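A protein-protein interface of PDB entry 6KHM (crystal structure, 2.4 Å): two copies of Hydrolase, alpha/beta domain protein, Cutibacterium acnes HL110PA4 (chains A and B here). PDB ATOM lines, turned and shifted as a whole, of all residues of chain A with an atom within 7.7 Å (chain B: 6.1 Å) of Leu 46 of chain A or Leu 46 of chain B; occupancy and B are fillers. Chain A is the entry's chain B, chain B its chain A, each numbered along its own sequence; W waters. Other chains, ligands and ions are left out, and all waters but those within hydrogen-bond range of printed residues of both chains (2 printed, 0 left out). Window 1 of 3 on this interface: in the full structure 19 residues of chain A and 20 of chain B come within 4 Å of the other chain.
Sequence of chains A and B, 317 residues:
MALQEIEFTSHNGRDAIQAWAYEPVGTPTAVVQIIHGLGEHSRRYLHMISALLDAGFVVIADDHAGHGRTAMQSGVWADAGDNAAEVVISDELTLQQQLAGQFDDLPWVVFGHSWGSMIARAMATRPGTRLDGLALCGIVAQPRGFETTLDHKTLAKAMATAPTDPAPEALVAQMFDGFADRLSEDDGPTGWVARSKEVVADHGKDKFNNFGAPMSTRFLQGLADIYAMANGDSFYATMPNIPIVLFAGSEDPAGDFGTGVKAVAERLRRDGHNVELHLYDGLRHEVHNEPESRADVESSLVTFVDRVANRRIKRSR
A ring nitrogen (ND1) of His 47 of chain A is in hydrogen-bond range of the side-chain carboxylate (OE2) of Glu 298 of chain A, 2.8 Å away.
Among the printed residues, merely in contact across the chains: Leu 46 of chain A with Leu 46 of chain B (3.1 Å), Asp 54 of chain A with His 47 of chain B (3.2 Å), Leu 3 of chain A with Arg 43 of chain B (3.4 Å), His 47 of chain A with Ser 50 of chain B (3.6 Å), Ser 50 of chain A with His 47 of chain B (3.7 Å), Tyr 22 of chain A with Leu 46 of chain B (3.7 Å), Leu 46 of chain A with Leu 53 of chain B (3.8 Å), Leu 53 of chain A with Leu 46 of chain B (3.9 Å), Leu 46 of chain A with Ser 50 of chain B (3.9 Å) and Leu 46 of chain A with Tyr 22 of chain B (3.9 Å).
His 41 of chain A touches none of the printed residues of chain B.
Tyr 45 of chain A touches none of the printed residues of chain B.
Of the printed residues of chain B, Leu 46 of chain A touches Tyr 22 (3.9 Å), Leu 46 (3.1 Å), Ser 50 (3.9 Å) and Leu 53 (3.8 Å).
Of the printed residues of chain B, His 47 of chain A touches Ser 50 (3.6 Å).
Of the printed residues of chain B, Ser 50 of chain A touches His 47.
Leu 46 of chain B touches just these residues of chain A: Tyr 22 (3.7 Å), Leu 46 (3.1 Å) and Leu 53 (3.9 Å).
The nearest residue of chain A that does not touch Leu 46 of chain B is Ser 50 of chain A (4.04 Å).
The nearest printed residue of chain A that does not touch Tyr 22 of chain B is Arg 43 of chain A (6.4 Å).
Printed residues of chain B that touch a printed residue of chain A: Tyr 22, Arg 43, Leu 46, His 47, Ser 50 and Leu 53.
Hydrophobic or aromatic side chains of chain B that line the printed part of chain A: Tyr 22, Leu 46, His 47 and Leu 53.
Among the printed residues, 10 pairs touch across the chains.
Among the printed residues, no Asp or Glu carboxylate lies within 4 Å of a Lys or Arg side-chain nitrogen of the other chain.
Leu 46 of chain A touches its own counterpart, Leu 46 of chain B.
Leu 46 of chain A touches Ser 50 of chain B, but with the chains exchanged Ser 50 of chain A does not touch Leu 46 of chain B (4.04 Å).
Leu 46 of chain A touches Leu 53 of chain B, and with the chains exchanged Leu 53 of chain A touches Leu 46 of chain B.
His 47 of chain A touches Ser 50 of chain B, and with the chains exchanged Ser 50 of chain A touches His 47 of chain B.
Positions printed for both chains: 22, 42, 43, 44, 45, 46, 47, 48, 49, 50, 51 and 53.
Of the 10 pairs that touch across the chains among the printed residues, 7 have their exchanged pair printed and touching as well.
Water W1 lies within hydrogen-bond range of OG of Ser 50 of chain A (2.5 Å), OD2 of Asp 54 of chain A (2.7 Å) and NE2 of His 47 of chain B (3.5 Å).
Water W2 bridges the guanidinium group (NH1) of Arg 43 of chain A (2.9 Å) and the guanidinium group (NH1) of Arg 43 of chain B (3.0 Å).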
ATOM      1  N   ALA A   2     -15.814 -17.267  20.172  1.00  0.00           N
ATOM      2  CA  ALA A   2     -16.888 -16.760  21.104  1.00  0.00           C
ATOM      3  C   ALA A   2     -16.357 -15.567  21.899  1.00  0.00           C
ATOM      4  O   ALA A   2     -15.204 -15.616  22.296  1.00  0.00           O
ATOM      5  CB  ALA A   2     -17.374 -17.868  22.031  1.00  0.00           C
ATOM      6  N   LEU A   3     -17.152 -14.519  22.066  1.00  0.00           N
ATOM      7  CA  LEU A   3     -16.726 -13.280  22.764  1.00  0.00           C
ATOM      8  C   LEU A   3     -17.673 -13.066  23.919  1.00  0.00           C
ATOM      9  O   LEU A   3     -18.859 -13.319  23.734  1.00  0.00           O
ATOM     10  CB  LEU A   3     -16.816 -12.094  21.817  1.00  0.00           C
ATOM     11  CG  LEU A   3     -16.396 -10.750  22.412  1.00  0.00           C
ATOM     12  CD1 LEU A   3     -14.956 -10.797  22.861  1.00  0.00           C
ATOM     13  CD2 LEU A   3     -16.561  -9.653  21.373  1.00  0.00           C
ATOM     14  N   ALA A  21     -13.661 -11.650  27.526  1.00  0.00           N
ATOM     15  CA  ALA A  21     -13.155 -13.038  27.473  1.00  0.00           C
ATOM     16  C   ALA A  21     -13.270 -13.509  26.017  1.00  0.00           C
ATOM     17  O   ALA A  21     -14.268 -13.292  25.387  1.00  0.00           O
ATOM     18  CB  ALA A  21     -13.873 -13.913  28.485  1.00  0.00           C
ATOM     19  N   TYR A  22     -12.194 -14.014  25.466  1.00  0.00           N
ATOM     20  CA  TYR A  22     -12.148 -14.547  24.088  1.00  0.00           C
ATOM     21  C   TYR A  22     -11.988 -16.062  24.200  1.00  0.00           C
ATOM     22  O   TYR A  22     -11.049 -16.480  24.864  1.00  0.00           O
ATOM     23  CB  TYR A  22     -10.974 -13.900  23.353  1.00  0.00           C
ATOM     24  CG  TYR A  22     -10.873 -12.397  23.471  1.00  0.00           C
ATOM     25  CD1 TYR A  22     -10.205 -11.799  24.521  1.00  0.00           C
ATOM     26  CD2 TYR A  22     -11.422 -11.579  22.500  1.00  0.00           C
ATOM     27  CE1 TYR A  22     -10.073 -10.425  24.600  1.00  0.00           C
ATOM     28  CE2 TYR A  22     -11.303 -10.198  22.564  1.00  0.00           C
ATOM     29  CZ  TYR A  22     -10.620  -9.625  23.616  1.00  0.00           C
ATOM     30  OH  TYR A  22     -10.528  -8.279  23.687  1.00  0.00           O
ATOM     31  N   GLU A  23     -12.932 -16.840  23.682  1.00  0.00           N
ATOM     32  CA  GLU A  23     -12.831 -18.317  23.698  1.00  0.00           C
ATOM     33  C   GLU A  23     -12.542 -18.825  22.289  1.00  0.00           C
ATOM     34  O   GLU A  23     -13.138 -18.387  21.324  1.00  0.00           O
ATOM     35  CB  GLU A  23     -14.116 -18.951  24.239  1.00  0.00           C
ATOM     36  CG  GLU A  23     -14.615 -18.316  25.529  1.00  0.00           C
ATOM     37  CD  GLU A  23     -15.973 -18.846  25.937  1.00  0.00           C
ATOM     38  OE1 GLU A  23     -16.252 -20.030  25.682  1.00  0.00           O
ATOM     39  OE2 GLU A  23     -16.727 -18.086  26.502  1.00  0.00           O
ATOM     40  N   ILE A  34      -4.343 -11.584  30.382  1.00  0.00           N
ATOM     41  CA  ILE A  34      -3.363 -10.531  29.987  1.00  0.00           C
ATOM     42  C   ILE A  34      -3.597  -9.341  30.921  1.00  0.00           C
ATOM     43  O   ILE A  34      -4.734  -8.959  31.052  1.00  0.00           O
ATOM     44  CB  ILE A  34      -3.508 -10.158  28.499  1.00  0.00           C
ATOM     45  CG1 ILE A  34      -3.114 -11.351  27.647  1.00  0.00           C
ATOM     46  CG2 ILE A  34      -2.696  -8.923  28.123  1.00  0.00           C
ATOM     47  CD1 ILE A  34      -3.437 -11.144  26.181  1.00  0.00           C
ATOM     48  N   HIS A  41      -3.770  -0.369  27.081  1.00  0.00           N
ATOM     49  CA  HIS A  41      -5.078  -1.046  27.259  1.00  0.00           C
ATOM     50  C   HIS A  41      -4.990  -2.474  26.730  1.00  0.00           C
ATOM     51  O   HIS A  41      -4.017  -2.774  25.983  1.00  0.00           O
ATOM     52  CB  HIS A  41      -6.183  -0.271  26.510  1.00  0.00           C
ATOM     53  CG  HIS A  41      -5.975  -0.165  25.039  1.00  0.00           C
ATOM     54  ND1 HIS A  41      -6.738  -0.862  24.133  1.00  0.00           N
ATOM     55  CD2 HIS A  41      -5.086   0.539  24.318  1.00  0.00           C
ATOM     56  CE1 HIS A  41      -6.312  -0.601  22.913  1.00  0.00           C
ATOM     57  NE2 HIS A  41      -5.285   0.245  22.995  1.00  0.00           N
ATOM     58  N   SER A  42      -5.990  -3.296  27.042  1.00  0.00           N
ATOM     59  CA  SER A  42      -6.000  -4.763  26.770  1.00  0.00           C
ATOM     60  C   SER A  42      -6.213  -5.047  25.269  1.00  0.00           C
ATOM     61  O   SER A  42      -5.760  -6.120  24.821  1.00  0.00           O
ATOM     62  CB  SER A  42      -7.071  -5.422  27.571  1.00  0.00           C
ATOM     63  OG  SER A  42      -8.318  -4.919  27.140  1.00  0.00           O
ATOM     64  N   ARG A  43      -6.887  -4.164  24.525  1.00  0.00           N
ATOM     65  CA  ARG A  43      -7.268  -4.433  23.109  1.00  0.00           C
ATOM     66  C   ARG A  43      -6.101  -4.134  22.151  1.00  0.00           C
ATOM     67  O   ARG A  43      -6.181  -4.474  20.978  1.00  0.00           O
ATOM     68  CB  ARG A  43      -8.553  -3.685  22.765  1.00  0.00           C
ATOM     69  CG  ARG A  43      -9.747  -4.290  23.493  1.00  0.00           C
ATOM     70  CD  ARG A  43     -11.066  -3.706  23.120  1.00  0.00           C
ATOM     71  NE  ARG A  43     -11.159  -2.301  23.478  1.00  0.00           N
ATOM     72  CZ  ARG A  43     -12.176  -1.524  23.123  1.00  0.00           C
ATOM     73  NH1 ARG A  43     -13.185  -2.012  22.419  1.00  0.00           N
ATOM     74  NH2 ARG A  43     -12.178  -0.258  23.465  1.00  0.00           N
ATOM     75  N   ARG A  44      -5.050  -3.521  22.662  1.00  0.00           N
ATOM     76  CA  ARG A  44      -3.727  -3.412  22.013  1.00  0.00           C
ATOM     77  C   ARG A  44      -3.097  -4.795  21.793  1.00  0.00           C
ATOM     78  O   ARG A  44      -2.239  -4.887  20.916  1.00  0.00           O
ATOM     79  CB  ARG A  44      -2.840  -2.543  22.910  1.00  0.00           C
ATOM     80  CG  ARG A  44      -1.561  -2.054  22.260  1.00  0.00           C
ATOM     81  CD  ARG A  44      -1.046  -0.793  22.948  1.00  0.00           C
ATOM     82  NE  ARG A  44       0.156  -0.386  22.252  1.00  0.00           N
ATOM     83  CZ  ARG A  44       1.377  -0.383  22.761  1.00  0.00           C
ATOM     84  NH1 ARG A  44       1.581  -0.684  24.036  1.00  0.00           N
ATOM     85  NH2 ARG A  44       2.398   0.001  22.004  1.00  0.00           N
ATOM     86  N   TYR A  45      -3.506  -5.824  22.545  1.00  0.00           N
ATOM     87  CA  TYR A  45      -2.918  -7.192  22.520  1.00  0.00           C
ATOM     88  C   TYR A  45      -3.614  -8.049  21.442  1.00  0.00           C
ATOM     89  O   TYR A  45      -3.626  -9.278  21.549  1.00  0.00           O
ATOM     90  CB  TYR A  45      -2.967  -7.785  23.945  1.00  0.00           C
ATOM     91  CG  TYR A  45      -1.998  -7.135  24.911  1.00  0.00           C
ATOM     92  CD1 TYR A  45      -2.225  -5.870  25.413  1.00  0.00           C
ATOM     93  CD2 TYR A  45      -0.807  -7.751  25.252  1.00  0.00           C
ATOM     94  CE1 TYR A  45      -1.297  -5.235  26.220  1.00  0.00           C
ATOM     95  CE2 TYR A  45       0.126  -7.136  26.077  1.00  0.00           C
ATOM     96  CZ  TYR A  45      -0.120  -5.873  26.564  1.00  0.00           C
ATOM     97  OH  TYR A  45       0.786  -5.258  27.376  1.00  0.00           O
ATOM     98  N   LEU A  46      -4.205  -7.426  20.428  1.00  0.00           N
ATOM     99  CA  LEU A  46      -4.990  -8.111  19.375  1.00  0.00           C
ATOM    100  C   LEU A  46      -4.136  -9.217  18.710  1.00  0.00           C
ATOM    101  O   LEU A  46      -4.593 -10.374  18.661  1.00  0.00           O
ATOM    102  CB  LEU A  46      -5.475  -7.012  18.426  1.00  0.00           C
ATOM    103  CG  LEU A  46      -6.056  -7.408  17.066  1.00  0.00           C
ATOM    104  CD1 LEU A  46      -6.677  -8.785  17.075  1.00  0.00           C
ATOM    105  CD2 LEU A  46      -7.079  -6.373  16.643  1.00  0.00           C
ATOM    106  N   HIS A  47      -2.921  -8.937  18.253  1.00  0.00           N
ATOM    107  CA  HIS A  47      -2.067  -9.976  17.624  1.00  0.00           C
ATOM    108  C   HIS A  47      -1.851 -11.128  18.620  1.00  0.00           C
ATOM    109  O   HIS A  47      -1.976 -12.270  18.211  1.00  0.00           O
ATOM    110  CB  HIS A  47      -0.752  -9.381  17.090  1.00  0.00           C
ATOM    111  CG  HIS A  47       0.019 -10.325  16.226  1.00  0.00           C
ATOM    112  ND1 HIS A  47       0.766 -11.386  16.755  1.00  0.00           N
ATOM    113  CD2 HIS A  47       0.151 -10.380  14.883  1.00  0.00           C
ATOM    114  CE1 HIS A  47       1.324 -12.050  15.760  1.00  0.00           C
ATOM    115  NE2 HIS A  47       0.956 -11.455  14.597  1.00  0.00           N
ATOM    116  N   MET A  48      -1.552 -10.844  19.887  1.00  0.00           N
ATOM    117  CA  MET A  48      -1.242 -11.906  20.873  1.00  0.00           C
ATOM    118  C   MET A  48      -2.513 -12.676  21.267  1.00  0.00           C
ATOM    119  O   MET A  48      -2.442 -13.920  21.449  1.00  0.00           O
ATOM    120  CB  MET A  48      -0.575 -11.334  22.123  1.00  0.00           C
ATOM    121  CG  MET A  48      -0.309 -12.428  23.143  1.00  0.00           C
ATOM    122  SD  MET A  48       0.327 -11.809  24.696  1.00  0.00           S
ATOM    123  CE  MET A  48       2.004 -11.386  24.224  1.00  0.00           C
ATOM    124  N   ILE A  49      -3.637 -11.980  21.445  1.00  0.00           N
ATOM    125  CA  ILE A  49      -4.956 -12.596  21.757  1.00  0.00           C
ATOM    126  C   ILE A  49      -5.276 -13.626  20.680  1.00  0.00           C
ATOM    127  O   ILE A  49      -5.535 -14.763  21.035  1.00  0.00           O
ATOM    128  CB  ILE A  49      -6.043 -11.522  21.887  1.00  0.00           C
ATOM    129  CG1 ILE A  49      -5.823 -10.664  23.143  1.00  0.00           C
ATOM    130  CG2 ILE A  49      -7.421 -12.152  21.865  1.00  0.00           C
ATOM    131  CD1 ILE A  49      -6.523  -9.327  23.093  1.00  0.00           C
ATOM    132  N   SER A  50      -5.219 -13.224  19.414  1.00  0.00           N
ATOM    133  CA  SER A  50      -5.432 -14.089  18.219  1.00  0.00           C
ATOM    134  C   SER A  50      -4.523 -15.311  18.274  1.00  0.00           C
ATOM    135  O   SER A  50      -5.010 -16.419  18.073  1.00  0.00           O
ATOM    136  CB  SER A  50      -5.200 -13.343  16.942  1.00  0.00           C
ATOM    137  OG  SER A  50      -5.822 -14.037  15.884  1.00  0.00           O
ATOM    138  N   ALA A  51      -3.240 -15.103  18.540  1.00  0.00           N
ATOM    139  CA  ALA A  51      -2.236 -16.188  18.524  1.00  0.00           C
ATOM    140  C   ALA A  51      -2.567 -17.183  19.643  1.00  0.00           C
ATOM    141  O   ALA A  51      -2.386 -18.364  19.426  1.00  0.00           O
ATOM    142  CB  ALA A  51      -0.835 -15.621  18.646  1.00  0.00           C
ATOM    143  N   LEU A  52      -3.096 -16.717  20.778  1.00  0.00           N
ATOM    144  CA  LEU A  52      -3.377 -17.591  21.944  1.00  0.00           C
ATOM    145  C   LEU A  52      -4.663 -18.376  21.682  1.00  0.00           C
ATOM    146  O   LEU A  52      -4.771 -19.541  22.167  1.00  0.00           O
ATOM    147  CB  LEU A  52      -3.448 -16.753  23.217  1.00  0.00           C
ATOM    148  CG  LEU A  52      -2.112 -16.177  23.671  1.00  0.00           C
ATOM    149  CD1 LEU A  52      -2.295 -15.286  24.882  1.00  0.00           C
ATOM    150  CD2 LEU A  52      -1.113 -17.288  23.979  1.00  0.00           C
ATOM    151  N   LEU A  53      -5.586 -17.776  20.931  1.00  0.00           N
ATOM    152  CA  LEU A  53      -6.834 -18.448  20.498  1.00  0.00           C
ATOM    153  C   LEU A  53      -6.488 -19.548  19.500  1.00  0.00           C
ATOM    154  O   LEU A  53      -7.044 -20.644  19.663  1.00  0.00           O
ATOM    155  CB  LEU A  53      -7.807 -17.445  19.878  1.00  0.00           C
ATOM    156  CG  LEU A  53      -8.476 -16.458  20.830  1.00  0.00           C
ATOM    157  CD1 LEU A  53      -9.389 -15.549  20.019  1.00  0.00           C
ATOM    158  CD2 LEU A  53      -9.278 -17.151  21.898  1.00  0.00           C
ATOM    159  N   ASP A  54      -5.602 -19.275  18.526  1.00  0.00           N
ATOM    160  CA  ASP A  54      -5.163 -20.272  17.503  1.00  0.00           C
ATOM    161  C   ASP A  54      -4.584 -21.492  18.228  1.00  0.00           C
ATOM    162  O   ASP A  54      -4.814 -22.606  17.750  1.00  0.00           O
ATOM    163  CB  ASP A  54      -4.113 -19.727  16.524  1.00  0.00           C
ATOM    164  CG  ASP A  54      -4.573 -18.570  15.643  1.00  0.00           C
ATOM    165  OD1 ASP A  54      -5.814 -18.338  15.564  1.00  0.00           O
ATOM    166  OD2 ASP A  54      -3.667 -17.880  15.066  1.00  0.00           O
ATOM    167  N   ASN A 289       5.804  -6.352  21.106  1.00  0.00           N
ATOM    168  CA  ASN A 289       5.286  -5.559  19.955  1.00  0.00           C
ATOM    169  C   ASN A 289       6.405  -5.310  18.941  1.00  0.00           C
ATOM    170  O   ASN A 289       6.036  -4.991  17.800  1.00  0.00           O
ATOM    171  CB  ASN A 289       4.621  -4.248  20.376  1.00  0.00           C
ATOM    172  CG  ASN A 289       3.353  -4.463  21.168  1.00  0.00           C
ATOM    173  OD1 ASN A 289       2.577  -5.393  20.893  1.00  0.00           O
ATOM    174  ND2 ASN A 289       3.146  -3.599  22.158  1.00  0.00           N
ATOM    175  N   ARG A 294       8.347 -10.158  18.283  1.00  0.00           N
ATOM    176  CA  ARG A 294       6.932 -10.471  18.608  1.00  0.00           C
ATOM    177  C   ARG A 294       6.670 -11.979  18.461  1.00  0.00           C
ATOM    178  O   ARG A 294       6.073 -12.568  19.401  1.00  0.00           O
ATOM    179  CB  ARG A 294       5.942  -9.691  17.739  1.00  0.00           C
ATOM    180  CG  ARG A 294       4.507 -10.142  17.971  1.00  0.00           C
ATOM    181  CD  ARG A 294       3.515  -9.083  17.613  1.00  0.00           C
ATOM    182  NE  ARG A 294       3.501  -9.013  16.169  1.00  0.00           N
ATOM    183  CZ  ARG A 294       2.802  -8.135  15.476  1.00  0.00           C
ATOM    184  NH1 ARG A 294       2.052  -7.255  16.120  1.00  0.00           N
ATOM    185  NH2 ARG A 294       2.863  -8.151  14.151  1.00  0.00           N
ATOM    186  N   GLU A 298       5.494 -14.707  21.379  1.00  0.00           N
ATOM    187  CA  GLU A 298       4.172 -15.392  21.284  1.00  0.00           C
ATOM    188  C   GLU A 298       4.419 -16.892  21.204  1.00  0.00           C
ATOM    189  O   GLU A 298       3.735 -17.610  21.894  1.00  0.00           O
ATOM    190  CB  GLU A 298       3.358 -14.895  20.088  1.00  0.00           C
ATOM    191  CG  GLU A 298       3.016 -13.441  20.235  1.00  0.00           C
ATOM    192  CD  GLU A 298       2.174 -12.845  19.133  1.00  0.00           C
ATOM    193  OE1 GLU A 298       2.104 -13.481  18.047  1.00  0.00           O
ATOM    194  OE2 GLU A 298       1.612 -11.719  19.370  1.00  0.00           O
ATOM    195  N   TYR B  22      -9.555  -0.522  13.064  1.00  0.00           N
ATOM    196  CA  TYR B  22      -8.268  -1.092  13.544  1.00  0.00           C
ATOM    197  C   TYR B  22      -7.178  -0.560  12.635  1.00  0.00           C
ATOM    198  O   TYR B  22      -7.258  -0.858  11.428  1.00  0.00           O
ATOM    199  CB  TYR B  22      -8.321  -2.616  13.535  1.00  0.00           C
ATOM    200  CG  TYR B  22      -9.541  -3.189  14.211  1.00  0.00           C
ATOM    201  CD1 TYR B  22      -9.545  -3.488  15.564  1.00  0.00           C
ATOM    202  CD2 TYR B  22     -10.697  -3.439  13.493  1.00  0.00           C
ATOM    203  CE1 TYR B  22     -10.653  -4.043  16.181  1.00  0.00           C
ATOM    204  CE2 TYR B  22     -11.827  -3.953  14.105  1.00  0.00           C
ATOM    205  CZ  TYR B  22     -11.791  -4.292  15.442  1.00  0.00           C
ATOM    206  OH  TYR B  22     -12.891  -4.804  16.039  1.00  0.00           O
ATOM    207  N   SER B  42     -19.036  -8.617  13.839  1.00  0.00           N
ATOM    208  CA  SER B  42     -17.761  -8.153  13.217  1.00  0.00           C
ATOM    209  C   SER B  42     -16.535  -8.533  14.066  1.00  0.00           C
ATOM    210  O   SER B  42     -15.449  -8.659  13.487  1.00  0.00           O
ATOM    211  CB  SER B  42     -17.825  -6.685  13.010  1.00  0.00           C
ATOM    212  OG  SER B  42     -17.659  -5.980  14.235  1.00  0.00           O
ATOM    213  N   ARG B  43     -16.678  -8.700  15.382  1.00  0.00           N
ATOM    214  CA  ARG B  43     -15.547  -9.114  16.267  1.00  0.00           C
ATOM    215  C   ARG B  43     -15.347 -10.640  16.214  1.00  0.00           C
ATOM    216  O   ARG B  43     -14.467 -11.120  16.896  1.00  0.00           O
ATOM    217  CB  ARG B  43     -15.739  -8.553  17.676  1.00  0.00           C
ATOM    218  CG  ARG B  43     -15.515  -7.049  17.739  1.00  0.00           C
ATOM    219  CD  ARG B  43     -15.756  -6.419  19.102  1.00  0.00           C
ATOM    220  NE  ARG B  43     -17.076  -6.693  19.640  1.00  0.00           N
ATOM    221  CZ  ARG B  43     -17.452  -6.429  20.894  1.00  0.00           C
ATOM    222  NH1 ARG B  43     -16.603  -5.882  21.760  1.00  0.00           N
ATOM    223  NH2 ARG B  43     -18.681  -6.757  21.286  1.00  0.00           N
ATOM    224  N   ARG B  44     -16.122 -11.364  15.411  1.00  0.00           N
ATOM    225  CA  ARG B  44     -15.904 -12.798  15.128  1.00  0.00           C
ATOM    226  C   ARG B  44     -14.740 -12.930  14.134  1.00  0.00           C
ATOM    227  O   ARG B  44     -14.143 -14.018  14.054  1.00  0.00           O
ATOM    228  CB  ARG B  44     -17.215 -13.399  14.614  1.00  0.00           C
ATOM    229  CG  ARG B  44     -17.181 -14.908  14.432  1.00  0.00           C
ATOM    230  CD  ARG B  44     -18.569 -15.465  14.259  1.00  0.00           C
ATOM    231  NE  ARG B  44     -18.500 -16.896  14.027  1.00  0.00           N
ATOM    232  CZ  ARG B  44     -19.002 -17.534  12.971  1.00  0.00           C
ATOM    233  NH1 ARG B  44     -19.701 -16.896  12.044  1.00  0.00           N
ATOM    234  NH2 ARG B  44     -18.863 -18.842  12.888  1.00  0.00           N
ATOM    235  N   TYR B  45     -14.399 -11.840  13.440  1.00  0.00           N
ATOM    236  CA  TYR B  45     -13.343 -11.761  12.397  1.00  0.00           C
ATOM    237  C   TYR B  45     -11.980 -11.445  13.046  1.00  0.00           C
ATOM    238  O   TYR B  45     -11.062 -11.012  12.336  1.00  0.00           O
ATOM    239  CB  TYR B  45     -13.746 -10.736  11.320  1.00  0.00           C
ATOM    240  CG  TYR B  45     -14.921 -11.189  10.495  1.00  0.00           C
ATOM    241  CD1 TYR B  45     -16.215 -11.100  10.977  1.00  0.00           C
ATOM    242  CD2 TYR B  45     -14.724 -11.834   9.288  1.00  0.00           C
ATOM    243  CE1 TYR B  45     -17.283 -11.600  10.253  1.00  0.00           C
ATOM    244  CE2 TYR B  45     -15.780 -12.310   8.537  1.00  0.00           C
ATOM    245  CZ  TYR B  45     -17.072 -12.198   9.019  1.00  0.00           C
ATOM    246  OH  TYR B  45     -18.112 -12.717   8.292  1.00  0.00           O
ATOM    247  N   LEU B  46     -11.836 -11.688  14.344  1.00  0.00           N
ATOM    248  CA  LEU B  46     -10.567 -11.445  15.090  1.00  0.00           C
ATOM    249  C   LEU B  46      -9.339 -11.918  14.284  1.00  0.00           C
ATOM    250  O   LEU B  46      -8.472 -11.086  14.012  1.00  0.00           O
ATOM    251  CB  LEU B  46     -10.665 -12.130  16.457  1.00  0.00           C
ATOM    252  CG  LEU B  46     -10.078 -11.327  17.612  1.00  0.00           C
ATOM    253  CD1 LEU B  46     -10.404 -11.960  18.961  1.00  0.00           C
ATOM    254  CD2 LEU B  46      -8.579 -11.179  17.437  1.00  0.00           C
ATOM    255  N   HIS B  47      -9.275 -13.193  13.905  1.00  0.00           N
ATOM    256  CA  HIS B  47      -8.189 -13.776  13.076  1.00  0.00           C
ATOM    257  C   HIS B  47      -8.000 -12.977  11.789  1.00  0.00           C
ATOM    258  O   HIS B  47      -6.849 -12.741  11.415  1.00  0.00           O
ATOM    259  CB  HIS B  47      -8.459 -15.253  12.691  1.00  0.00           C
ATOM    260  CG  HIS B  47      -7.231 -15.967  12.222  1.00  0.00           C
ATOM    261  ND1 HIS B  47      -6.839 -15.963  10.891  1.00  0.00           N
ATOM    262  CD2 HIS B  47      -6.290 -16.685  12.889  1.00  0.00           C
ATOM    263  CE1 HIS B  47      -5.708 -16.635  10.751  1.00  0.00           C
ATOM    264  NE2 HIS B  47      -5.351 -17.106  11.962  1.00  0.00           N
ATOM    265  N   MET B  48      -9.075 -12.647  11.073  1.00  0.00           N
ATOM    266  CA  MET B  48      -8.910 -12.020   9.739  1.00  0.00           C
ATOM    267  C   MET B  48      -8.400 -10.587   9.966  1.00  0.00           C
ATOM    268  O   MET B  48      -7.374 -10.204   9.345  1.00  0.00           O
ATOM    269  CB  MET B  48     -10.210 -12.043   8.935  1.00  0.00           C
ATOM    270  CG  MET B  48     -10.045 -11.462   7.553  1.00  0.00           C
ATOM    271  SD  MET B  48     -11.612 -11.295   6.624  1.00  0.00           S
ATOM    272  CE  MET B  48     -11.550 -12.918   5.871  1.00  0.00           C
ATOM    273  N   ILE B  49      -9.041  -9.857  10.875  1.00  0.00           N
ATOM    274  CA  ILE B  49      -8.652  -8.481  11.296  1.00  0.00           C
ATOM    275  C   ILE B  49      -7.151  -8.445  11.592  1.00  0.00           C
ATOM    276  O   ILE B  49      -6.434  -7.660  10.991  1.00  0.00           O
ATOM    277  CB  ILE B  49      -9.469  -8.037  12.519  1.00  0.00           C
ATOM    278  CG1 ILE B  49     -10.954  -7.872  12.161  1.00  0.00           C
ATOM    279  CG2 ILE B  49      -8.880  -6.763  13.077  1.00  0.00           C
ATOM    280  CD1 ILE B  49     -11.904  -7.651  13.343  1.00  0.00           C
ATOM    281  N   SER B  50      -6.683  -9.326  12.461  1.00  0.00           N
ATOM    282  CA  SER B  50      -5.250  -9.404  12.829  1.00  0.00           C
ATOM    283  C   SER B  50      -4.401  -9.710  11.579  1.00  0.00           C
ATOM    284  O   SER B  50      -3.344  -9.046  11.411  1.00  0.00           O
ATOM    285  CB  SER B  50      -5.075 -10.407  13.925  1.00  0.00           C
ATOM    286  OG  SER B  50      -3.760 -10.386  14.427  1.00  0.00           O
ATOM    287  N   ALA B  51      -4.832 -10.638  10.711  1.00  0.00           N
ATOM    288  CA  ALA B  51      -4.093 -11.010   9.471  1.00  0.00           C
ATOM    289  C   ALA B  51      -4.000  -9.789   8.555  1.00  0.00           C
ATOM    290  O   ALA B  51      -2.952  -9.612   7.919  1.00  0.00           O
ATOM    291  CB  ALA B  51      -4.738 -12.159   8.724  1.00  0.00           C
ATOM    292  N   LEU B  53      -4.182  -6.474   9.470  1.00  0.00           N
ATOM    293  CA  LEU B  53      -3.282  -5.516  10.151  1.00  0.00           C
ATOM    294  C   LEU B  53      -1.839  -5.948   9.857  1.00  0.00           C
ATOM    295  O   LEU B  53      -1.026  -5.083   9.465  1.00  0.00           O
ATOM    296  CB  LEU B  53      -3.607  -5.470  11.647  1.00  0.00           C
ATOM    297  CG  LEU B  53      -4.897  -4.751  12.070  1.00  0.00           C
ATOM    298  CD1 LEU B  53      -5.293  -5.143  13.500  1.00  0.00           C
ATOM    299  CD2 LEU B  53      -4.762  -3.224  11.990  1.00  0.00           C
HETATM  300  O   HOH W   1      -4.021 -15.235  14.577  1.00  0.00           O
HETATM  301  O   HOH W   2     -13.840  -4.644  21.450  1.00  0.00           O
